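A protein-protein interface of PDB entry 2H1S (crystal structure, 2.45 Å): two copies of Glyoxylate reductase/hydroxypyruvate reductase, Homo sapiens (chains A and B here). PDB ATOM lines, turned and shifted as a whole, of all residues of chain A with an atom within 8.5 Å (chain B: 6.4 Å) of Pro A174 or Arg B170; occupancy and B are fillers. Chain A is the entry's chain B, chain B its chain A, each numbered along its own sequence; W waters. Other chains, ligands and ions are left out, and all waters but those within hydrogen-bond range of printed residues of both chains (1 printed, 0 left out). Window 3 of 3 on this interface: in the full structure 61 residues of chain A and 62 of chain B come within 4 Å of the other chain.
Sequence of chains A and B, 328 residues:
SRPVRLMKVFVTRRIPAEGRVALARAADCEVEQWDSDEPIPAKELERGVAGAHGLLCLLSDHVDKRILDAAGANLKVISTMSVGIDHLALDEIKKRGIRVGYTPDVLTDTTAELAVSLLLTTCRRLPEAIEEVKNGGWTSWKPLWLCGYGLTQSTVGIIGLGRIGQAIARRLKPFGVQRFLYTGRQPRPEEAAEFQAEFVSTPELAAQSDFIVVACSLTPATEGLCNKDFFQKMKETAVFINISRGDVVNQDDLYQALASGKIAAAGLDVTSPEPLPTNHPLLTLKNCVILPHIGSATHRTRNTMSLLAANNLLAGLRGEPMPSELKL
Water W1 lies within hydrogen-bond range of NH2 of Arg B171 (2.4 Å), OD1 of Asp B109 (3.3 Å) and O of Phe A175 (3.5 Å).
Arg A170 touches Pro B174, and with the chains exchanged Pro A174 touches Arg B170. Arg A171 touches Pro B174, and with the chains exchanged Pro A174 touches Arg B171. Arg A171 touches Phe B175, and with the chains exchanged Phe A175 touches Arg B171. Pro A174 touches its own counterpart, Pro B174. 10 positions are printed for both chains. Of the 8 pairs that touch across the chains among the printed residues, 7 have their exchanged pair printed and touching as well.
Of the printed residues of chain B, Pro A174 touches Arg B170 (3.3 Å), Arg B171 (3.5 Å) and Pro B174 (3.3 Å). Of the printed residues of chain B, Phe A175 touches Arg B171. Arg B170 touches just one residue of chain A: Pro A174 (3.3 Å). Of the printed residues of chain A, Phe B175 touches Arg A171. The nearest residue of chain A that does not touch Arg B170 is Phe A175 (6.1 Å).
Of the 17 printed residues of chain B, 5 touch a printed residue of chain A. Hydrophobic or aromatic side chains of chain B that line the printed part of chain A: Pro B174 and Phe B175. Of the 14 printed residues of chain A, 5 touch a printed residue of chain B. Hydrophobic or aromatic side chains of chain A that line the printed part of chain B: Pro A174 and Phe A175.
The guanidinium group (NH1) of Arg A171 sits close to the backbone carbonyl oxygen (O) of Phe B175 (3.3 Å).
Thr A152 touches Asp B109. Arg A170 touches Pro B174 (O to CB, 3.3 Å). Arg A171 touches Pro B174. Pro A174 touches Arg B170 (CB to O, 3.3 Å). Pro A174 touches Arg B171. Pro A174 touches Pro B174. NH1 of Arg B171 touches CA of Phe A175 (3.6 Å).
NH2 of Arg B171 is in salt-bridge range of OD1 of Asp B109, 2.6 Å away. The backbone carbonyl oxygen (O) of Ala B167 is in hydrogen-bond range of the guanidinium group (NE) of Arg B171, 3.2 Å away. The guanidinium group of Arg B170 lies within salt-bridge range of the side-chain carboxylate of Glu B194.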
ATOM      1  N   LEU A 151       0.723  10.530 -25.931  1.00  0.00           N
ATOM      2  CA  LEU A 151       1.126   9.444 -26.815  1.00  0.00           C
ATOM      3  C   LEU A 151       1.136   8.088 -26.151  1.00  0.00           C
ATOM      4  O   LEU A 151       1.375   7.098 -26.813  1.00  0.00           O
ATOM      5  CB  LEU A 151       2.519   9.736 -27.331  1.00  0.00           C
ATOM      6  CG  LEU A 151       2.586  10.816 -28.392  1.00  0.00           C
ATOM      7  CD1 LEU A 151       3.937  11.457 -28.284  1.00  0.00           C
ATOM      8  CD2 LEU A 151       2.387  10.151 -29.746  1.00  0.00           C
ATOM      9  N   THR A 152       0.855   8.030 -24.859  1.00  0.00           N
ATOM     10  CA  THR A 152       0.876   6.761 -24.164  1.00  0.00           C
ATOM     11  C   THR A 152      -0.187   5.853 -24.771  1.00  0.00           C
ATOM     12  O   THR A 152      -1.348   6.245 -24.873  1.00  0.00           O
ATOM     13  CB  THR A 152       0.650   6.923 -22.629  1.00  0.00           C
ATOM     14  OG1 THR A 152       1.836   7.488 -22.053  1.00  0.00           O
ATOM     15  CG2 THR A 152       0.402   5.576 -21.964  1.00  0.00           C
ATOM     16  N   ILE A 168      10.491  10.246 -37.906  1.00  0.00           N
ATOM     17  CA  ILE A 168       9.440  10.688 -36.974  1.00  0.00           C
ATOM     18  C   ILE A 168       9.020   9.468 -36.144  1.00  0.00           C
ATOM     19  O   ILE A 168       9.051   9.509 -34.917  1.00  0.00           O
ATOM     20  CB  ILE A 168       8.230  11.370 -37.687  1.00  0.00           C
ATOM     21  CG1 ILE A 168       8.696  12.638 -38.386  1.00  0.00           C
ATOM     22  CG2 ILE A 168       7.108  11.703 -36.693  1.00  0.00           C
ATOM     23  CD1 ILE A 168       7.656  13.206 -39.280  1.00  0.00           C
ATOM     24  N   ALA A 169       8.678   8.373 -36.823  1.00  0.00           N
ATOM     25  CA  ALA A 169       8.331   7.152 -36.135  1.00  0.00           C
ATOM     26  C   ALA A 169       9.354   6.794 -35.052  1.00  0.00           C
ATOM     27  O   ALA A 169       8.985   6.475 -33.924  1.00  0.00           O
ATOM     28  CB  ALA A 169       8.194   6.028 -37.132  1.00  0.00           C
ATOM     29  N   ARG A 170      10.636   6.839 -35.385  1.00  0.00           N
ATOM     30  CA  ARG A 170      11.695   6.409 -34.468  1.00  0.00           C
ATOM     31  C   ARG A 170      11.758   7.318 -33.209  1.00  0.00           C
ATOM     32  O   ARG A 170      11.978   6.835 -32.109  1.00  0.00           O
ATOM     33  CB  ARG A 170      13.029   6.325 -35.238  1.00  0.00           C
ATOM     34  CG  ARG A 170      14.240   5.734 -34.526  1.00  0.00           C
ATOM     35  CD  ARG A 170      15.492   5.769 -35.453  1.00  0.00           C
ATOM     36  NE  ARG A 170      15.234   5.107 -36.742  1.00  0.00           N
ATOM     37  CZ  ARG A 170      15.207   5.712 -37.939  1.00  0.00           C
ATOM     38  NH1 ARG A 170      15.423   7.022 -38.047  1.00  0.00           N
ATOM     39  NH2 ARG A 170      14.960   4.990 -39.042  1.00  0.00           N
ATOM     40  N   ARG A 171      11.512   8.611 -33.366  1.00  0.00           N
ATOM     41  CA  ARG A 171      11.468   9.514 -32.229  1.00  0.00           C
ATOM     42  C   ARG A 171      10.229   9.290 -31.358  1.00  0.00           C
ATOM     43  O   ARG A 171      10.288   9.406 -30.110  1.00  0.00           O
ATOM     44  CB  ARG A 171      11.601  10.952 -32.679  1.00  0.00           C
ATOM     45  CG  ARG A 171      12.934  11.139 -33.317  1.00  0.00           C
ATOM     46  CD  ARG A 171      13.370  12.539 -33.630  1.00  0.00           C
ATOM     47  NE  ARG A 171      14.376  12.348 -34.659  1.00  0.00           N
ATOM     48  CZ  ARG A 171      15.530  12.987 -34.764  1.00  0.00           C
ATOM     49  NH1 ARG A 171      15.916  13.928 -33.889  1.00  0.00           N
ATOM     50  NH2 ARG A 171      16.314  12.649 -35.763  1.00  0.00           N
ATOM     51  N   LEU A 172       9.133   8.906 -31.995  1.00  0.00           N
ATOM     52  CA  LEU A 172       7.901   8.771 -31.264  1.00  0.00           C
ATOM     53  C   LEU A 172       7.795   7.442 -30.499  1.00  0.00           C
ATOM     54  O   LEU A 172       7.134   7.355 -29.465  1.00  0.00           O
ATOM     55  CB  LEU A 172       6.723   8.969 -32.216  1.00  0.00           C
ATOM     56  CG  LEU A 172       6.433  10.348 -32.772  1.00  0.00           C
ATOM     57  CD1 LEU A 172       5.281  10.143 -33.746  1.00  0.00           C
ATOM     58  CD2 LEU A 172       6.045  11.384 -31.659  1.00  0.00           C
ATOM     59  N   LYS A 173       8.420   6.399 -31.006  1.00  0.00           N
ATOM     60  CA  LYS A 173       8.314   5.099 -30.353  1.00  0.00           C
ATOM     61  C   LYS A 173       8.463   5.169 -28.801  1.00  0.00           C
ATOM     62  O   LYS A 173       7.564   4.689 -28.073  1.00  0.00           O
ATOM     63  CB  LYS A 173       9.309   4.130 -30.980  1.00  0.00           C
ATOM     64  CG  LYS A 173       9.219   2.696 -30.539  1.00  0.00           C
ATOM     65  CD  LYS A 173      10.279   1.861 -31.245  1.00  0.00           C
ATOM     66  CE  LYS A 173      10.085   0.356 -30.951  1.00  0.00           C
ATOM     67  NZ  LYS A 173      11.290  -0.493 -31.263  1.00  0.00           N
ATOM     68  N   PRO A 174       9.565   5.761 -28.269  1.00  0.00           N
ATOM     69  CA  PRO A 174       9.640   5.672 -26.791  1.00  0.00           C
ATOM     70  C   PRO A 174       8.703   6.595 -25.991  1.00  0.00           C
ATOM     71  O   PRO A 174       8.712   6.557 -24.777  1.00  0.00           O
ATOM     72  CB  PRO A 174      11.126   5.913 -26.485  1.00  0.00           C
ATOM     73  CG  PRO A 174      11.607   6.715 -27.633  1.00  0.00           C
ATOM     74  CD  PRO A 174      10.743   6.446 -28.837  1.00  0.00           C
ATOM     75  N   PHE A 175       7.874   7.398 -26.642  1.00  0.00           N
ATOM     76  CA  PHE A 175       6.788   8.039 -25.912  1.00  0.00           C
ATOM     77  C   PHE A 175       5.612   7.088 -25.606  1.00  0.00           C
ATOM     78  O   PHE A 175       4.621   7.508 -25.019  1.00  0.00           O
ATOM     79  CB  PHE A 175       6.255   9.188 -26.712  1.00  0.00           C
ATOM     80  CG  PHE A 175       7.190  10.337 -26.814  1.00  0.00           C
ATOM     81  CD1 PHE A 175       8.296  10.280 -27.670  1.00  0.00           C
ATOM     82  CD2 PHE A 175       6.947  11.500 -26.104  1.00  0.00           C
ATOM     83  CE1 PHE A 175       9.131  11.347 -27.795  1.00  0.00           C
ATOM     84  CE2 PHE A 175       7.793  12.594 -26.235  1.00  0.00           C
ATOM     85  CZ  PHE A 175       8.881  12.517 -27.074  1.00  0.00           C
ATOM     86  N   GLY A 176       5.710   5.822 -26.019  1.00  0.00           N
ATOM     87  CA  GLY A 176       4.726   4.817 -25.599  1.00  0.00           C
ATOM     88  C   GLY A 176       3.680   4.504 -26.644  1.00  0.00           C
ATOM     89  O   GLY A 176       2.646   3.918 -26.348  1.00  0.00           O
ATOM     90  N   VAL A 177       3.943   4.894 -27.875  1.00  0.00           N
ATOM     91  CA  VAL A 177       3.113   4.492 -28.997  1.00  0.00           C
ATOM     92  C   VAL A 177       2.970   2.962 -29.056  1.00  0.00           C
ATOM     93  O   VAL A 177       3.956   2.223 -29.055  1.00  0.00           O
ATOM     94  CB  VAL A 177       3.709   5.010 -30.312  1.00  0.00           C
ATOM     95  CG1 VAL A 177       2.833   4.628 -31.493  1.00  0.00           C
ATOM     96  CG2 VAL A 177       3.918   6.513 -30.234  1.00  0.00           C
ATOM     97  N   PHE A 180       1.918   1.763 -34.991  1.00  0.00           N
ATOM     98  CA  PHE A 180       2.177   2.703 -36.098  1.00  0.00           C
ATOM     99  C   PHE A 180       1.466   2.246 -37.351  1.00  0.00           C
ATOM    100  O   PHE A 180       1.522   1.078 -37.702  1.00  0.00           O
ATOM    101  CB  PHE A 180       3.645   2.783 -36.411  1.00  0.00           C
ATOM    102  CG  PHE A 180       4.450   3.481 -35.377  1.00  0.00           C
ATOM    103  CD1 PHE A 180       4.660   4.846 -35.458  1.00  0.00           C
ATOM    104  CD2 PHE A 180       5.069   2.755 -34.359  1.00  0.00           C
ATOM    105  CE1 PHE A 180       5.454   5.492 -34.513  1.00  0.00           C
ATOM    106  CE2 PHE A 180       5.848   3.378 -33.425  1.00  0.00           C
ATOM    107  CZ  PHE A 180       6.045   4.753 -33.498  1.00  0.00           C
ATOM    108  N   PHE A 195       9.537  -0.565 -36.887  1.00  0.00           N
ATOM    109  CA  PHE A 195       8.437   0.024 -36.101  1.00  0.00           C
ATOM    110  C   PHE A 195       7.232  -0.888 -36.058  1.00  0.00           C
ATOM    111  O   PHE A 195       6.212  -0.531 -35.503  1.00  0.00           O
ATOM    112  CB  PHE A 195       7.980   1.342 -36.720  1.00  0.00           C
ATOM    113  CG  PHE A 195       9.097   2.215 -37.135  1.00  0.00           C
ATOM    114  CD1 PHE A 195       9.915   2.816 -36.183  1.00  0.00           C
ATOM    115  CD2 PHE A 195       9.350   2.435 -38.486  1.00  0.00           C
ATOM    116  CE1 PHE A 195      10.963   3.627 -36.562  1.00  0.00           C
ATOM    117  CE2 PHE A 195      10.389   3.256 -38.878  1.00  0.00           C
ATOM    118  CZ  PHE A 195      11.207   3.848 -37.908  1.00  0.00           C
ATOM    119  N   THR B 108       4.417   9.690 -14.390  1.00  0.00           N
ATOM    120  CA  THR B 108       5.762   9.620 -14.865  1.00  0.00           C
ATOM    121  C   THR B 108       5.804   9.897 -16.348  1.00  0.00           C
ATOM    122  O   THR B 108       6.469  10.839 -16.754  1.00  0.00           O
ATOM    123  CB  THR B 108       6.407   8.264 -14.557  1.00  0.00           C
ATOM    124  OG1 THR B 108       6.365   8.048 -13.140  1.00  0.00           O
ATOM    125  CG2 THR B 108       7.857   8.217 -15.022  1.00  0.00           C
ATOM    126  N   ASP B 109       5.081   9.122 -17.156  1.00  0.00           N
ATOM    127  CA  ASP B 109       5.171   9.261 -18.637  1.00  0.00           C
ATOM    128  C   ASP B 109       4.728  10.646 -19.163  1.00  0.00           C
ATOM    129  O   ASP B 109       5.400  11.284 -20.015  1.00  0.00           O
ATOM    130  CB  ASP B 109       4.358   8.166 -19.337  1.00  0.00           C
ATOM    131  CG  ASP B 109       4.994   6.771 -19.228  1.00  0.00           C
ATOM    132  OD1 ASP B 109       6.239   6.640 -19.202  1.00  0.00           O
ATOM    133  OD2 ASP B 109       4.232   5.780 -19.205  1.00  0.00           O
ATOM    134  N   ARG B 163      12.573   8.152 -11.634  1.00  0.00           N
ATOM    135  CA  ARG B 163      11.641   7.592 -12.601  1.00  0.00           C
ATOM    136  C   ARG B 163      11.355   8.596 -13.699  1.00  0.00           C
ATOM    137  O   ARG B 163      11.461   8.271 -14.894  1.00  0.00           O
ATOM    138  CB  ARG B 163      10.368   7.014 -11.936  1.00  0.00           C
ATOM    139  CG  ARG B 163      10.562   5.637 -11.212  1.00  0.00           C
ATOM    140  CD  ARG B 163      10.822   4.398 -12.149  1.00  0.00           C
ATOM    141  NE  ARG B 163      10.965   3.117 -11.426  1.00  0.00           N
ATOM    142  CZ  ARG B 163      12.127   2.481 -11.151  1.00  0.00           C
ATOM    143  NH1 ARG B 163      13.310   2.974 -11.528  1.00  0.00           N
ATOM    144  NH2 ARG B 163      12.125   1.319 -10.485  1.00  0.00           N
ATOM    145  N   GLY B 165      13.245  11.264 -14.668  1.00  0.00           N
ATOM    146  CA  GLY B 165      14.496  11.544 -15.409  1.00  0.00           C
ATOM    147  C   GLY B 165      14.815  10.450 -16.414  1.00  0.00           C
ATOM    148  O   GLY B 165      15.072  10.707 -17.604  1.00  0.00           O
ATOM    149  N   GLN B 166      14.774   9.221 -15.923  1.00  0.00           N
ATOM    150  CA  GLN B 166      14.869   8.014 -16.722  1.00  0.00           C
ATOM    151  C   GLN B 166      13.911   8.022 -17.907  1.00  0.00           C
ATOM    152  O   GLN B 166      14.304   7.649 -19.006  1.00  0.00           O
ATOM    153  CB  GLN B 166      14.517   6.806 -15.840  1.00  0.00           C
ATOM    154  CG  GLN B 166      15.626   6.363 -14.909  1.00  0.00           C
ATOM    155  CD  GLN B 166      15.100   5.743 -13.648  1.00  0.00           C
ATOM    156  OE1 GLN B 166      14.222   4.871 -13.679  1.00  0.00           O
ATOM    157  NE2 GLN B 166      15.632   6.185 -12.519  1.00  0.00           N
ATOM    158  N   ALA B 167      12.665   8.444 -17.673  1.00  0.00           N
ATOM    159  CA  ALA B 167      11.688   8.494 -18.732  1.00  0.00           C
ATOM    160  C   ALA B 167      11.933   9.676 -19.683  1.00  0.00           C
ATOM    161  O   ALA B 167      11.446   9.658 -20.832  1.00  0.00           O
ATOM    162  CB  ALA B 167      10.231   8.479 -18.157  1.00  0.00           C
ATOM    163  N   ILE B 168      12.680  10.685 -19.231  1.00  0.00           N
ATOM    164  CA  ILE B 168      13.088  11.766 -20.137  1.00  0.00           C
ATOM    165  C   ILE B 168      14.208  11.244 -21.041  1.00  0.00           C
ATOM    166  O   ILE B 168      14.137  11.353 -22.263  1.00  0.00           O
ATOM    167  CB  ILE B 168      13.507  13.065 -19.379  1.00  0.00           C
ATOM    168  CG1 ILE B 168      12.268  13.740 -18.816  1.00  0.00           C
ATOM    169  CG2 ILE B 168      14.364  14.046 -20.264  1.00  0.00           C
ATOM    170  CD1 ILE B 168      12.586  14.754 -17.728  1.00  0.00           C
ATOM    171  N   ALA B 169      15.217  10.638 -20.425  1.00  0.00           N
ATOM    172  CA  ALA B 169      16.341  10.060 -21.146  1.00  0.00           C
ATOM    173  C   ALA B 169      15.848   9.113 -22.245  1.00  0.00           C
ATOM    174  O   ALA B 169      16.310   9.178 -23.381  1.00  0.00           O
ATOM    175  CB  ALA B 169      17.289   9.327 -20.164  1.00  0.00           C
ATOM    176  N   ARG B 170      14.889   8.258 -21.891  1.00  0.00           N
ATOM    177  CA  ARG B 170      14.315   7.263 -22.794  1.00  0.00           C
ATOM    178  C   ARG B 170      13.649   7.895 -24.016  1.00  0.00           C
ATOM    179  O   ARG B 170      13.781   7.404 -25.117  1.00  0.00           O
ATOM    180  CB  ARG B 170      13.310   6.403 -22.003  1.00  0.00           C
ATOM    181  CG  ARG B 170      12.557   5.321 -22.770  1.00  0.00           C
ATOM    182  CD  ARG B 170      11.684   4.556 -21.810  1.00  0.00           C
ATOM    183  NE  ARG B 170      12.475   3.987 -20.709  1.00  0.00           N
ATOM    184  CZ  ARG B 170      12.198   4.146 -19.418  1.00  0.00           C
ATOM    185  NH1 ARG B 170      11.143   4.845 -19.022  1.00  0.00           N
ATOM    186  NH2 ARG B 170      12.965   3.577 -18.517  1.00  0.00           N
ATOM    187  N   ARG B 171      12.950   8.997 -23.832  1.00  0.00           N
ATOM    188  CA  ARG B 171      12.351   9.686 -24.971  1.00  0.00           C
ATOM    189  C   ARG B 171      13.399  10.456 -25.791  1.00  0.00           C
ATOM    190  O   ARG B 171      13.268  10.607 -27.029  1.00  0.00           O
ATOM    191  CB  ARG B 171      11.178  10.591 -24.542  1.00  0.00           C
ATOM    192  CG  ARG B 171       9.894   9.837 -24.241  1.00  0.00           C
ATOM    193  CD  ARG B 171       9.152  10.296 -22.951  1.00  0.00           C
ATOM    194  NE  ARG B 171       8.659   9.110 -22.226  1.00  0.00           N
ATOM    195  CZ  ARG B 171       7.375   8.768 -22.143  1.00  0.00           C
ATOM    196  NH1 ARG B 171       6.448   9.543 -22.690  1.00  0.00           N
ATOM    197  NH2 ARG B 171       7.010   7.663 -21.514  1.00  0.00           N
ATOM    198  N   LEU B 172      14.455  10.912 -25.125  1.00  0.00           N
ATOM    199  CA  LEU B 172      15.503  11.677 -25.823  1.00  0.00           C
ATOM    200  C   LEU B 172      16.474  10.840 -26.684  1.00  0.00           C
ATOM    201  O   LEU B 172      16.974  11.284 -27.708  1.00  0.00           O
ATOM    202  CB  LEU B 172      16.266  12.559 -24.817  1.00  0.00           C
ATOM    203  CG  LEU B 172      15.550  13.842 -24.363  1.00  0.00           C
ATOM    204  CD1 LEU B 172      16.403  14.642 -23.383  1.00  0.00           C
ATOM    205  CD2 LEU B 172      15.122  14.739 -25.543  1.00  0.00           C
ATOM    206  N   LYS B 173      16.725   9.610 -26.270  1.00  0.00           N
ATOM    207  CA  LYS B 173      17.713   8.780 -26.943  1.00  0.00           C
ATOM    208  C   LYS B 173      17.529   8.724 -28.483  1.00  0.00           C
ATOM    209  O   LYS B 173      18.499   8.961 -29.231  1.00  0.00           O
ATOM    210  CB  LYS B 173      17.740   7.397 -26.276  1.00  0.00           C
ATOM    211  CG  LYS B 173      18.730   6.373 -26.781  1.00  0.00           C
ATOM    212  CD  LYS B 173      18.560   5.107 -25.944  1.00  0.00           C
ATOM    213  CE  LYS B 173      19.116   3.844 -26.607  1.00  0.00           C
ATOM    214  NZ  LYS B 173      20.620   3.787 -26.607  1.00  0.00           N
ATOM    215  N   PRO B 174      16.311   8.427 -28.981  1.00  0.00           N
ATOM    216  CA  PRO B 174      16.165   8.372 -30.449  1.00  0.00           C
ATOM    217  C   PRO B 174      16.302   9.695 -31.225  1.00  0.00           C
ATOM    218  O   PRO B 174      16.316   9.678 -32.436  1.00  0.00           O
ATOM    219  CB  PRO B 174      14.759   7.797 -30.656  1.00  0.00           C
ATOM    220  CG  PRO B 174      14.397   7.184 -29.344  1.00  0.00           C
ATOM    221  CD  PRO B 174      15.052   8.059 -28.312  1.00  0.00           C
ATOM    222  N   PHE B 175      16.420  10.832 -30.551  1.00  0.00           N
ATOM    223  CA  PHE B 175      16.736  12.052 -31.280  1.00  0.00           C
ATOM    224  C   PHE B 175      18.222  12.147 -31.588  1.00  0.00           C
ATOM    225  O   PHE B 175      18.667  13.131 -32.154  1.00  0.00           O
ATOM    226  CB  PHE B 175      16.288  13.282 -30.498  1.00  0.00           C
ATOM    227  CG  PHE B 175      14.803  13.402 -30.357  1.00  0.00           C
ATOM    228  CD1 PHE B 175      14.089  12.509 -29.568  1.00  0.00           C
ATOM    229  CD2 PHE B 175      14.125  14.426 -30.991  1.00  0.00           C
ATOM    230  CE1 PHE B 175      12.734  12.625 -29.422  1.00  0.00           C
ATOM    231  CE2 PHE B 175      12.747  14.542 -30.843  1.00  0.00           C
ATOM    232  CZ  PHE B 175      12.062  13.619 -30.055  1.00  0.00           C
ATOM    233  N   PHE B 180      24.560  10.673 -22.302  1.00  0.00           N
ATOM    234  CA  PHE B 180      23.750  11.094 -21.186  1.00  0.00           C
ATOM    235  C   PHE B 180      24.610  11.198 -19.908  1.00  0.00           C
ATOM    236  O   PHE B 180      25.356  10.288 -19.564  1.00  0.00           O
ATOM    237  CB  PHE B 180      22.606  10.100 -20.959  1.00  0.00           C
ATOM    238  CG  PHE B 180      21.485  10.198 -21.955  1.00  0.00           C
ATOM    239  CD1 PHE B 180      20.650  11.322 -21.990  1.00  0.00           C
ATOM    240  CD2 PHE B 180      21.215   9.142 -22.825  1.00  0.00           C
ATOM    241  CE1 PHE B 180      19.560  11.414 -22.901  1.00  0.00           C
ATOM    242  CE2 PHE B 180      20.117   9.209 -23.742  1.00  0.00           C
ATOM    243  CZ  PHE B 180      19.290  10.362 -23.780  1.00  0.00           C
ATOM    244  N   GLU B 194      20.513   1.433 -19.011  1.00  0.00           N
ATOM    245  CA  GLU B 194      19.688   1.515 -20.224  1.00  0.00           C
ATOM    246  C   GLU B 194      20.161   2.617 -21.189  1.00  0.00           C
ATOM    247  O   GLU B 194      19.985   2.496 -22.401  1.00  0.00           O
ATOM    248  CB  GLU B 194      18.192   1.694 -19.873  1.00  0.00           C
ATOM    249  CG  GLU B 194      17.302   2.217 -21.041  1.00  0.00           C
ATOM    250  CD  GLU B 194      15.782   2.172 -20.794  1.00  0.00           C
ATOM    251  OE1 GLU B 194      15.311   2.444 -19.669  1.00  0.00           O
ATOM    252  OE2 GLU B 194      15.047   1.900 -21.765  1.00  0.00           O
ATOM    253  N   PHE B 195      20.772   3.672 -20.656  1.00  0.00           N
ATOM    254  CA  PHE B 195      21.152   4.836 -21.462  1.00  0.00           C
ATOM    255  C   PHE B 195      22.662   5.028 -21.480  1.00  0.00           C
ATOM    256  O   PHE B 195      23.168   5.992 -22.052  1.00  0.00           O
ATOM    257  CB  PHE B 195      20.492   6.103 -20.908  1.00  0.00           C
ATOM    258  CG  PHE B 195      19.136   5.864 -20.308  1.00  0.00           C
ATOM    259  CD1 PHE B 195      18.010   5.705 -21.123  1.00  0.00           C
ATOM    260  CD2 PHE B 195      18.976   5.796 -18.909  1.00  0.00           C
ATOM    261  CE1 PHE B 195      16.748   5.491 -20.558  1.00  0.00           C
ATOM    262  CE2 PHE B 195      17.705   5.580 -18.330  1.00  0.00           C
ATOM    263  CZ  PHE B 195      16.597   5.414 -19.158  1.00  0.00           C
HETATM  264  O   HOH W   1       5.882   5.698 -22.329  1.00  0.00           O
